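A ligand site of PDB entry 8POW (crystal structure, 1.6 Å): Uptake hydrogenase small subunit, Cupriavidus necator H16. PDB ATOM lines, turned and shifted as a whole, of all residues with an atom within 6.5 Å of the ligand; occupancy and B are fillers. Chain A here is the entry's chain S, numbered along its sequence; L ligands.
The backbone NH of Arg 192 sits close to the side-chain sulfur of Cys 190. NH2 of Arg 193 lies within hydrogen-bond range of O of His 187 (3.0 Å). The backbone carbonyl oxygen (O) of Gly 223 lies within hydrogen-bond range of the backbone NH (N) of His 187. SG of Cys 215 sits close to N of Tyr 217 (3.4 Å). N of Cys 221 is in hydrogen-bond range of O of Leu 216 (3.2 Å). The side-chain sulfur (SG) of Cys 221 lies close to the backbone NH (N) of Gly 223, 3.5 Å away. NE of Arg 192 sits at hydrogen-bond distance from OH of Tyr 191 (3.0 Å). The backbone carbonyl oxygen (O) of Phe 214 is in hydrogen-bond range of the guanidinium group (NH1) of Arg 192.
Arg 192 touches the ligand. Phe 196 touches the ligand (CB to S1, 3.9 Å). Tyr 217 touches the ligand. CA of Gly 223 touches S2 of the ligand, at 3.8 Å. CD of Pro 224 touches S3 of the ligand, 3.9 Å away. Ile 243 touches the ligand (CG2 to S4, 3.6 Å).
A ring nitrogen (ND1) of His 187 binds an iron atom (FE4) of the ligand. An iron atom (FE2) of the ligand is bound by the side-chain sulfur (SG) of Cys 215 (2.3 Å). The side-chain sulfur (SG) of Cys 221 binds an iron atom (FE1) of the ligand, 2.3 Å away. The backbone NH (N) of Arg 193 sits close to a sulfur (S1) of the ligand (3.5 Å). FE3 of the ligand is bound by SG of Cys 190. N of Leu 216 sits close to S4 of the ligand (3.4 Å).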
ATOM      1  N   ILE A 186     -21.414  16.836  36.551  1.00  0.00           N
ATOM      2  CA  ILE A 186     -20.810  15.522  36.271  1.00  0.00           C
ATOM      3  C   ILE A 186     -19.785  15.636  35.124  1.00  0.00           C
ATOM      4  O   ILE A 186     -18.676  15.087  35.187  1.00  0.00           O
ATOM      5  CB  ILE A 186     -21.879  14.466  35.858  1.00  0.00           C
ATOM      6  CG1 ILE A 186     -22.989  14.306  36.898  1.00  0.00           C
ATOM      7  CG2 ILE A 186     -21.239  13.112  35.538  1.00  0.00           C
ATOM      8  CD1 ILE A 186     -22.511  13.962  38.288  1.00  0.00           C
ATOM      9  N   HIS A 187     -20.193  16.361  34.098  1.00  0.00           N
ATOM     10  CA  HIS A 187     -19.408  16.602  32.868  1.00  0.00           C
ATOM     11  C   HIS A 187     -18.068  17.311  33.084  1.00  0.00           C
ATOM     12  O   HIS A 187     -17.151  17.146  32.263  1.00  0.00           O
ATOM     13  CB  HIS A 187     -20.291  17.428  31.931  1.00  0.00           C
ATOM     14  CG  HIS A 187     -19.760  17.592  30.544  1.00  0.00           C
ATOM     15  ND1 HIS A 187     -19.820  16.593  29.599  1.00  0.00           N
ATOM     16  CD2 HIS A 187     -19.209  18.664  29.925  1.00  0.00           C
ATOM     17  CE1 HIS A 187     -19.309  17.036  28.472  1.00  0.00           C
ATOM     18  NE2 HIS A 187     -18.931  18.282  28.636  1.00  0.00           N
ATOM     19  N   ASP A 188     -17.938  18.085  34.169  1.00  0.00           N
ATOM     20  CA  ASP A 188     -16.715  18.839  34.447  1.00  0.00           C
ATOM     21  C   ASP A 188     -15.487  17.928  34.584  1.00  0.00           C
ATOM     22  O   ASP A 188     -14.467  18.154  33.928  1.00  0.00           O
ATOM     23  CB  ASP A 188     -16.851  19.692  35.717  1.00  0.00           C
ATOM     24  CG  ASP A 188     -17.877  20.833  35.583  1.00  0.00           C
ATOM     25  OD1 ASP A 188     -18.300  21.173  34.464  1.00  0.00           O
ATOM     26  OD2 ASP A 188     -18.282  21.387  36.632  1.00  0.00           O
ATOM     27  N   CYS A 190     -15.759  14.318  34.457  1.00  0.00           N
ATOM     28  CA  CYS A 190     -16.021  12.980  33.892  1.00  0.00           C
ATOM     29  C   CYS A 190     -14.789  12.456  33.143  1.00  0.00           C
ATOM     30  O   CYS A 190     -14.251  13.149  32.297  1.00  0.00           O
ATOM     31  CB  CYS A 190     -17.218  12.993  32.950  1.00  0.00           C
ATOM     32  SG  CYS A 190     -17.592  11.368  32.253  1.00  0.00           S
ATOM     33  N   TYR A 191     -14.358  11.225  33.462  1.00  0.00           N
ATOM     34  CA  TYR A 191     -13.175  10.639  32.822  1.00  0.00           C
ATOM     35  C   TYR A 191     -13.340  10.442  31.310  1.00  0.00           C
ATOM     36  O   TYR A 191     -12.348  10.280  30.616  1.00  0.00           O
ATOM     37  CB  TYR A 191     -12.763   9.306  33.495  1.00  0.00           C
ATOM     38  CG  TYR A 191     -13.537   8.103  33.017  1.00  0.00           C
ATOM     39  CD1 TYR A 191     -14.865   7.912  33.412  1.00  0.00           C
ATOM     40  CD2 TYR A 191     -12.955   7.147  32.178  1.00  0.00           C
ATOM     41  CE1 TYR A 191     -15.583   6.813  32.978  1.00  0.00           C
ATOM     42  CE2 TYR A 191     -13.670   6.041  31.750  1.00  0.00           C
ATOM     43  CZ  TYR A 191     -14.986   5.885  32.148  1.00  0.00           C
ATOM     44  OH  TYR A 191     -15.710   4.808  31.726  1.00  0.00           O
ATOM     45  N   ARG A 192     -14.587  10.470  30.817  1.00  0.00           N
ATOM     46  CA  ARG A 192     -14.842  10.367  29.377  1.00  0.00           C
ATOM     47  C   ARG A 192     -14.792  11.739  28.662  1.00  0.00           C
ATOM     48  O   ARG A 192     -14.969  11.797  27.445  1.00  0.00           O
ATOM     49  CB  ARG A 192     -16.194   9.689  29.103  1.00  0.00           C
ATOM     50  CG  ARG A 192     -16.311   8.286  29.701  1.00  0.00           C
ATOM     51  CD  ARG A 192     -17.386   7.440  29.018  1.00  0.00           C
ATOM     52  NE  ARG A 192     -17.452   6.102  29.629  1.00  0.00           N
ATOM     53  CZ  ARG A 192     -17.984   5.006  29.060  1.00  0.00           C
ATOM     54  NH1 ARG A 192     -18.525   5.037  27.852  1.00  0.00           N
ATOM     55  NH2 ARG A 192     -17.967   3.851  29.726  1.00  0.00           N
ATOM     56  N   ARG A 193     -14.554  12.820  29.422  1.00  0.00           N
ATOM     57  CA  ARG A 193     -14.521  14.177  28.856  1.00  0.00           C
ATOM     58  C   ARG A 193     -13.536  14.348  27.685  1.00  0.00           C
ATOM     59  O   ARG A 193     -13.873  15.016  26.715  1.00  0.00           O
ATOM     60  CB  ARG A 193     -14.262  15.215  29.963  1.00  0.00           C
ATOM     61  CG  ARG A 193     -14.231  16.680  29.518  1.00  0.00           C
ATOM     62  CD  ARG A 193     -15.564  17.141  28.951  1.00  0.00           C
ATOM     63  NE  ARG A 193     -15.526  18.554  28.574  1.00  0.00           N
ATOM     64  CZ  ARG A 193     -15.627  19.575  29.425  1.00  0.00           C
ATOM     65  NH1 ARG A 193     -15.575  20.815  28.960  1.00  0.00           N
ATOM     66  NH2 ARG A 193     -15.763  19.372  30.733  1.00  0.00           N
ATOM     67  N   PRO A 194     -12.321  13.744  27.765  1.00  0.00           N
ATOM     68  CA  PRO A 194     -11.429  13.792  26.604  1.00  0.00           C
ATOM     69  C   PRO A 194     -12.053  13.258  25.312  1.00  0.00           C
ATOM     70  O   PRO A 194     -11.828  13.849  24.244  1.00  0.00           O
ATOM     71  CB  PRO A 194     -10.231  12.945  27.049  1.00  0.00           C
ATOM     72  CG  PRO A 194     -10.197  13.134  28.516  1.00  0.00           C
ATOM     73  CD  PRO A 194     -11.640  13.159  28.929  1.00  0.00           C
ATOM     74  N   HIS A 195     -12.831  12.177  25.407  1.00  0.00           N
ATOM     75  CA  HIS A 195     -13.565  11.664  24.246  1.00  0.00           C
ATOM     76  C   HIS A 195     -14.609  12.680  23.740  1.00  0.00           C
ATOM     77  O   HIS A 195     -14.707  12.938  22.532  1.00  0.00           O
ATOM     78  CB  HIS A 195     -14.236  10.314  24.541  1.00  0.00           C
ATOM     79  CG  HIS A 195     -13.259   9.197  24.770  1.00  0.00           C
ATOM     80  ND1 HIS A 195     -12.313   8.839  23.826  1.00  0.00           N
ATOM     81  CD2 HIS A 195     -13.105   8.352  25.809  1.00  0.00           C
ATOM     82  CE1 HIS A 195     -11.607   7.826  24.293  1.00  0.00           C
ATOM     83  NE2 HIS A 195     -12.068   7.508  25.494  1.00  0.00           N
ATOM     84  N   PHE A 196     -15.380  13.261  24.662  1.00  0.00           N
ATOM     85  CA  PHE A 196     -16.334  14.307  24.310  1.00  0.00           C
ATOM     86  C   PHE A 196     -15.654  15.437  23.542  1.00  0.00           C
ATOM     87  O   PHE A 196     -16.115  15.845  22.480  1.00  0.00           O
ATOM     88  CB  PHE A 196     -17.029  14.867  25.556  1.00  0.00           C
ATOM     89  CG  PHE A 196     -17.958  16.024  25.275  1.00  0.00           C
ATOM     90  CD1 PHE A 196     -19.296  15.806  25.000  1.00  0.00           C
ATOM     91  CD2 PHE A 196     -17.481  17.333  25.316  1.00  0.00           C
ATOM     92  CE1 PHE A 196     -20.156  16.870  24.749  1.00  0.00           C
ATOM     93  CE2 PHE A 196     -18.329  18.405  25.066  1.00  0.00           C
ATOM     94  CZ  PHE A 196     -19.675  18.173  24.779  1.00  0.00           C
ATOM     95  N   PHE A 201     -17.842   9.498  20.294  1.00  0.00           N
ATOM     96  CA  PHE A 201     -19.104   9.127  20.923  1.00  0.00           C
ATOM     97  C   PHE A 201     -19.564   7.703  20.605  1.00  0.00           C
ATOM     98  O   PHE A 201     -19.334   7.197  19.521  1.00  0.00           O
ATOM     99  CB  PHE A 201     -20.221  10.055  20.442  1.00  0.00           C
ATOM    100  CG  PHE A 201     -19.960  11.522  20.682  1.00  0.00           C
ATOM    101  CD1 PHE A 201     -20.091  12.049  21.955  1.00  0.00           C
ATOM    102  CD2 PHE A 201     -19.593  12.369  19.638  1.00  0.00           C
ATOM    103  CE1 PHE A 201     -19.855  13.396  22.181  1.00  0.00           C
ATOM    104  CE2 PHE A 201     -19.357  13.715  19.865  1.00  0.00           C
ATOM    105  CZ  PHE A 201     -19.485  14.235  21.143  1.00  0.00           C
ATOM    106  N   PHE A 214     -16.029   5.421  24.928  1.00  0.00           N
ATOM    107  CA  PHE A 214     -16.276   6.739  24.337  1.00  0.00           C
ATOM    108  C   PHE A 214     -17.428   7.434  25.078  1.00  0.00           C
ATOM    109  O   PHE A 214     -18.202   6.785  25.803  1.00  0.00           O
ATOM    110  CB  PHE A 214     -16.578   6.617  22.835  1.00  0.00           C
ATOM    111  CG  PHE A 214     -15.350   6.481  21.953  1.00  0.00           C
ATOM    112  CD1 PHE A 214     -14.101   6.184  22.468  1.00  0.00           C
ATOM    113  CD2 PHE A 214     -15.483   6.633  20.581  1.00  0.00           C
ATOM    114  CE1 PHE A 214     -12.990   6.059  21.624  1.00  0.00           C
ATOM    115  CE2 PHE A 214     -14.388   6.508  19.729  1.00  0.00           C
ATOM    116  CZ  PHE A 214     -13.141   6.224  20.262  1.00  0.00           C
ATOM    117  N   CYS A 215     -17.520   8.750  24.906  1.00  0.00           N
ATOM    118  CA  CYS A 215     -18.529   9.564  25.582  1.00  0.00           C
ATOM    119  C   CYS A 215     -19.964   9.135  25.226  1.00  0.00           C
ATOM    120  O   CYS A 215     -20.248   8.707  24.105  1.00  0.00           O
ATOM    121  CB  CYS A 215     -18.292  11.048  25.270  1.00  0.00           C
ATOM    122  SG  CYS A 215     -19.622  12.179  25.703  1.00  0.00           S
ATOM    123  N   LEU A 216     -20.857   9.244  26.221  1.00  0.00           N
ATOM    124  CA  LEU A 216     -22.226   8.756  26.111  1.00  0.00           C
ATOM    125  C   LEU A 216     -23.259   9.854  25.825  1.00  0.00           C
ATOM    126  O   LEU A 216     -24.473   9.621  25.937  1.00  0.00           O
ATOM    127  CB  LEU A 216     -22.595   8.031  27.416  1.00  0.00           C
ATOM    128  CG  LEU A 216     -21.732   6.788  27.717  1.00  0.00           C
ATOM    129  CD1 LEU A 216     -21.891   6.337  29.162  1.00  0.00           C
ATOM    130  CD2 LEU A 216     -22.094   5.641  26.782  1.00  0.00           C
ATOM    131  N   TYR A 217     -22.796  11.041  25.442  1.00  0.00           N
ATOM    132  CA  TYR A 217     -23.671  12.186  25.112  1.00  0.00           C
ATOM    133  C   TYR A 217     -24.760  11.808  24.108  1.00  0.00           C
ATOM    134  O   TYR A 217     -25.931  12.153  24.297  1.00  0.00           O
ATOM    135  CB  TYR A 217     -22.836  13.339  24.549  1.00  0.00           C
ATOM    136  CG  TYR A 217     -23.601  14.617  24.298  1.00  0.00           C
ATOM    137  CD1 TYR A 217     -23.850  15.507  25.340  1.00  0.00           C
ATOM    138  CD2 TYR A 217     -24.064  14.942  23.029  1.00  0.00           C
ATOM    139  CE1 TYR A 217     -24.546  16.693  25.119  1.00  0.00           C
ATOM    140  CE2 TYR A 217     -24.759  16.115  22.791  1.00  0.00           C
ATOM    141  CZ  TYR A 217     -24.996  16.998  23.834  1.00  0.00           C
ATOM    142  OH  TYR A 217     -25.690  18.157  23.594  1.00  0.00           O
ATOM    143  N   LYS A 218     -24.392  11.098  23.044  1.00  0.00           N
ATOM    144  CA  LYS A 218     -25.363  10.753  21.987  1.00  0.00           C
ATOM    145  C   LYS A 218     -26.304   9.613  22.392  1.00  0.00           C
ATOM    146  O   LYS A 218     -27.281   9.335  21.703  1.00  0.00           O
ATOM    147  CB  LYS A 218     -24.645  10.458  20.663  1.00  0.00           C
ATOM    148  CG  LYS A 218     -23.894  11.651  20.118  1.00  0.00           C
ATOM    149  CD  LYS A 218     -23.355  11.377  18.727  1.00  0.00           C
ATOM    150  CE  LYS A 218     -22.834  12.641  18.074  1.00  0.00           C
ATOM    151  NZ  LYS A 218     -22.227  12.323  16.757  1.00  0.00           N
ATOM    152  N   CYS A 221     -26.699  10.978  27.724  1.00  0.00           N
ATOM    153  CA  CYS A 221     -26.053  11.372  28.982  1.00  0.00           C
ATOM    154  C   CYS A 221     -26.384  12.821  29.360  1.00  0.00           C
ATOM    155  O   CYS A 221     -26.170  13.753  28.574  1.00  0.00           O
ATOM    156  CB  CYS A 221     -24.532  11.199  28.905  1.00  0.00           C
ATOM    157  SG  CYS A 221     -23.723  11.553  30.477  1.00  0.00           S
ATOM    158  N   LYS A 222     -26.890  12.990  30.580  1.00  0.00           N
ATOM    159  CA  LYS A 222     -27.286  14.320  31.074  1.00  0.00           C
ATOM    160  C   LYS A 222     -26.240  14.934  32.004  1.00  0.00           C
ATOM    161  O   LYS A 222     -26.498  15.947  32.669  1.00  0.00           O
ATOM    162  CB  LYS A 222     -28.658  14.264  31.738  1.00  0.00           C
ATOM    163  CG  LYS A 222     -29.790  13.774  30.830  1.00  0.00           C
ATOM    164  CD  LYS A 222     -29.806  14.486  29.482  1.00  0.00           C
ATOM    165  CE  LYS A 222     -31.073  14.173  28.693  1.00  0.00           C
ATOM    166  NZ  LYS A 222     -31.279  12.725  28.371  1.00  0.00           N
ATOM    167  N   GLY A 223     -25.058  14.339  32.031  1.00  0.00           N
ATOM    168  CA  GLY A 223     -23.953  14.884  32.800  1.00  0.00           C
ATOM    169  C   GLY A 223     -23.672  16.371  32.602  1.00  0.00           C
ATOM    170  O   GLY A 223     -23.323  17.063  33.579  1.00  0.00           O
ATOM    171  N   PRO A 224     -23.799  16.879  31.346  1.00  0.00           N
ATOM    172  CA  PRO A 224     -23.562  18.316  31.131  1.00  0.00           C
ATOM    173  C   PRO A 224     -24.490  19.293  31.838  1.00  0.00           C
ATOM    174  O   PRO A 224     -24.138  20.462  31.973  1.00  0.00           O
ATOM    175  CB  PRO A 224     -23.687  18.467  29.614  1.00  0.00           C
ATOM    176  CG  PRO A 224     -23.308  17.132  29.072  1.00  0.00           C
ATOM    177  CD  PRO A 224     -23.901  16.163  30.058  1.00  0.00           C
ATOM    178  N   PHE A 241     -19.307   4.697  38.785  1.00  0.00           N
ATOM    179  CA  PHE A 241     -20.478   5.570  38.720  1.00  0.00           C
ATOM    180  C   PHE A 241     -21.185   5.234  37.401  1.00  0.00           C
ATOM    181  O   PHE A 241     -20.641   4.503  36.575  1.00  0.00           O
ATOM    182  CB  PHE A 241     -20.109   7.053  38.946  1.00  0.00           C
ATOM    183  CG  PHE A 241     -19.395   7.728  37.789  1.00  0.00           C
ATOM    184  CD1 PHE A 241     -18.111   7.331  37.392  1.00  0.00           C
ATOM    185  CD2 PHE A 241     -19.967   8.822  37.162  1.00  0.00           C
ATOM    186  CE1 PHE A 241     -17.451   7.978  36.356  1.00  0.00           C
ATOM    187  CE2 PHE A 241     -19.307   9.483  36.127  1.00  0.00           C
ATOM    188  CZ  PHE A 241     -18.060   9.064  35.726  1.00  0.00           C
ATOM    189  N   ILE A 243     -21.741   6.406  34.431  1.00  0.00           N
ATOM    190  CA  ILE A 243     -20.994   6.562  33.170  1.00  0.00           C
ATOM    191  C   ILE A 243     -19.845   5.561  33.070  1.00  0.00           C
ATOM    192  O   ILE A 243     -19.622   4.970  32.005  1.00  0.00           O
ATOM    193  CB  ILE A 243     -20.519   8.023  33.004  1.00  0.00           C
ATOM    194  CG1 ILE A 243     -21.731   8.900  32.675  1.00  0.00           C
ATOM    195  CG2 ILE A 243     -19.478   8.170  31.906  1.00  0.00           C
ATOM    196  CD1 ILE A 243     -21.620  10.324  33.168  1.00  0.00           C
ATOM    197  N   GLY A 248     -25.350   6.416  30.378  1.00  0.00           N
ATOM    198  CA  GLY A 248     -25.313   7.852  30.570  1.00  0.00           C
ATOM    199  C   GLY A 248     -25.971   8.254  31.887  1.00  0.00           C
ATOM    200  O   GLY A 248     -26.831   7.563  32.424  1.00  0.00           O
ATOM    201  N   CYS A 249     -25.535   9.393  32.416  1.00  0.00           N
ATOM    202  CA  CYS A 249     -26.243  10.017  33.508  1.00  0.00           C
ATOM    203  C   CYS A 249     -27.692  10.280  33.044  1.00  0.00           C
ATOM    204  O   CYS A 249     -27.902  10.709  31.917  1.00  0.00           O
ATOM    205  CB  CYS A 249     -25.545  11.307  33.902  1.00  0.00           C
ATOM    206  SG  CYS A 249     -26.357  12.326  35.143  1.00  0.00           S
HETATM  207 FE1  LIG L   1     -21.626  12.329  29.835  1.00  0.00          FE
HETATM  208 FE2  LIG L   1     -19.706  12.422  27.958  1.00  0.00          FE
HETATM  209 FE3  LIG L   1     -18.994  12.153  30.594  1.00  0.00          FE
HETATM  210 FE4  LIG L   1     -19.980  14.488  29.598  1.00  0.00          FE
HETATM  211  S1  LIG L   1     -17.999  13.515  29.079  1.00  0.00           S
HETATM  212  S2  LIG L   1     -20.607  13.510  31.549  1.00  0.00           S
HETATM  213  S3  LIG L   1     -21.569  13.804  28.099  1.00  0.00           S
HETATM  214  S4  LIG L   1     -20.165  10.625  29.304  1.00  0.00           S
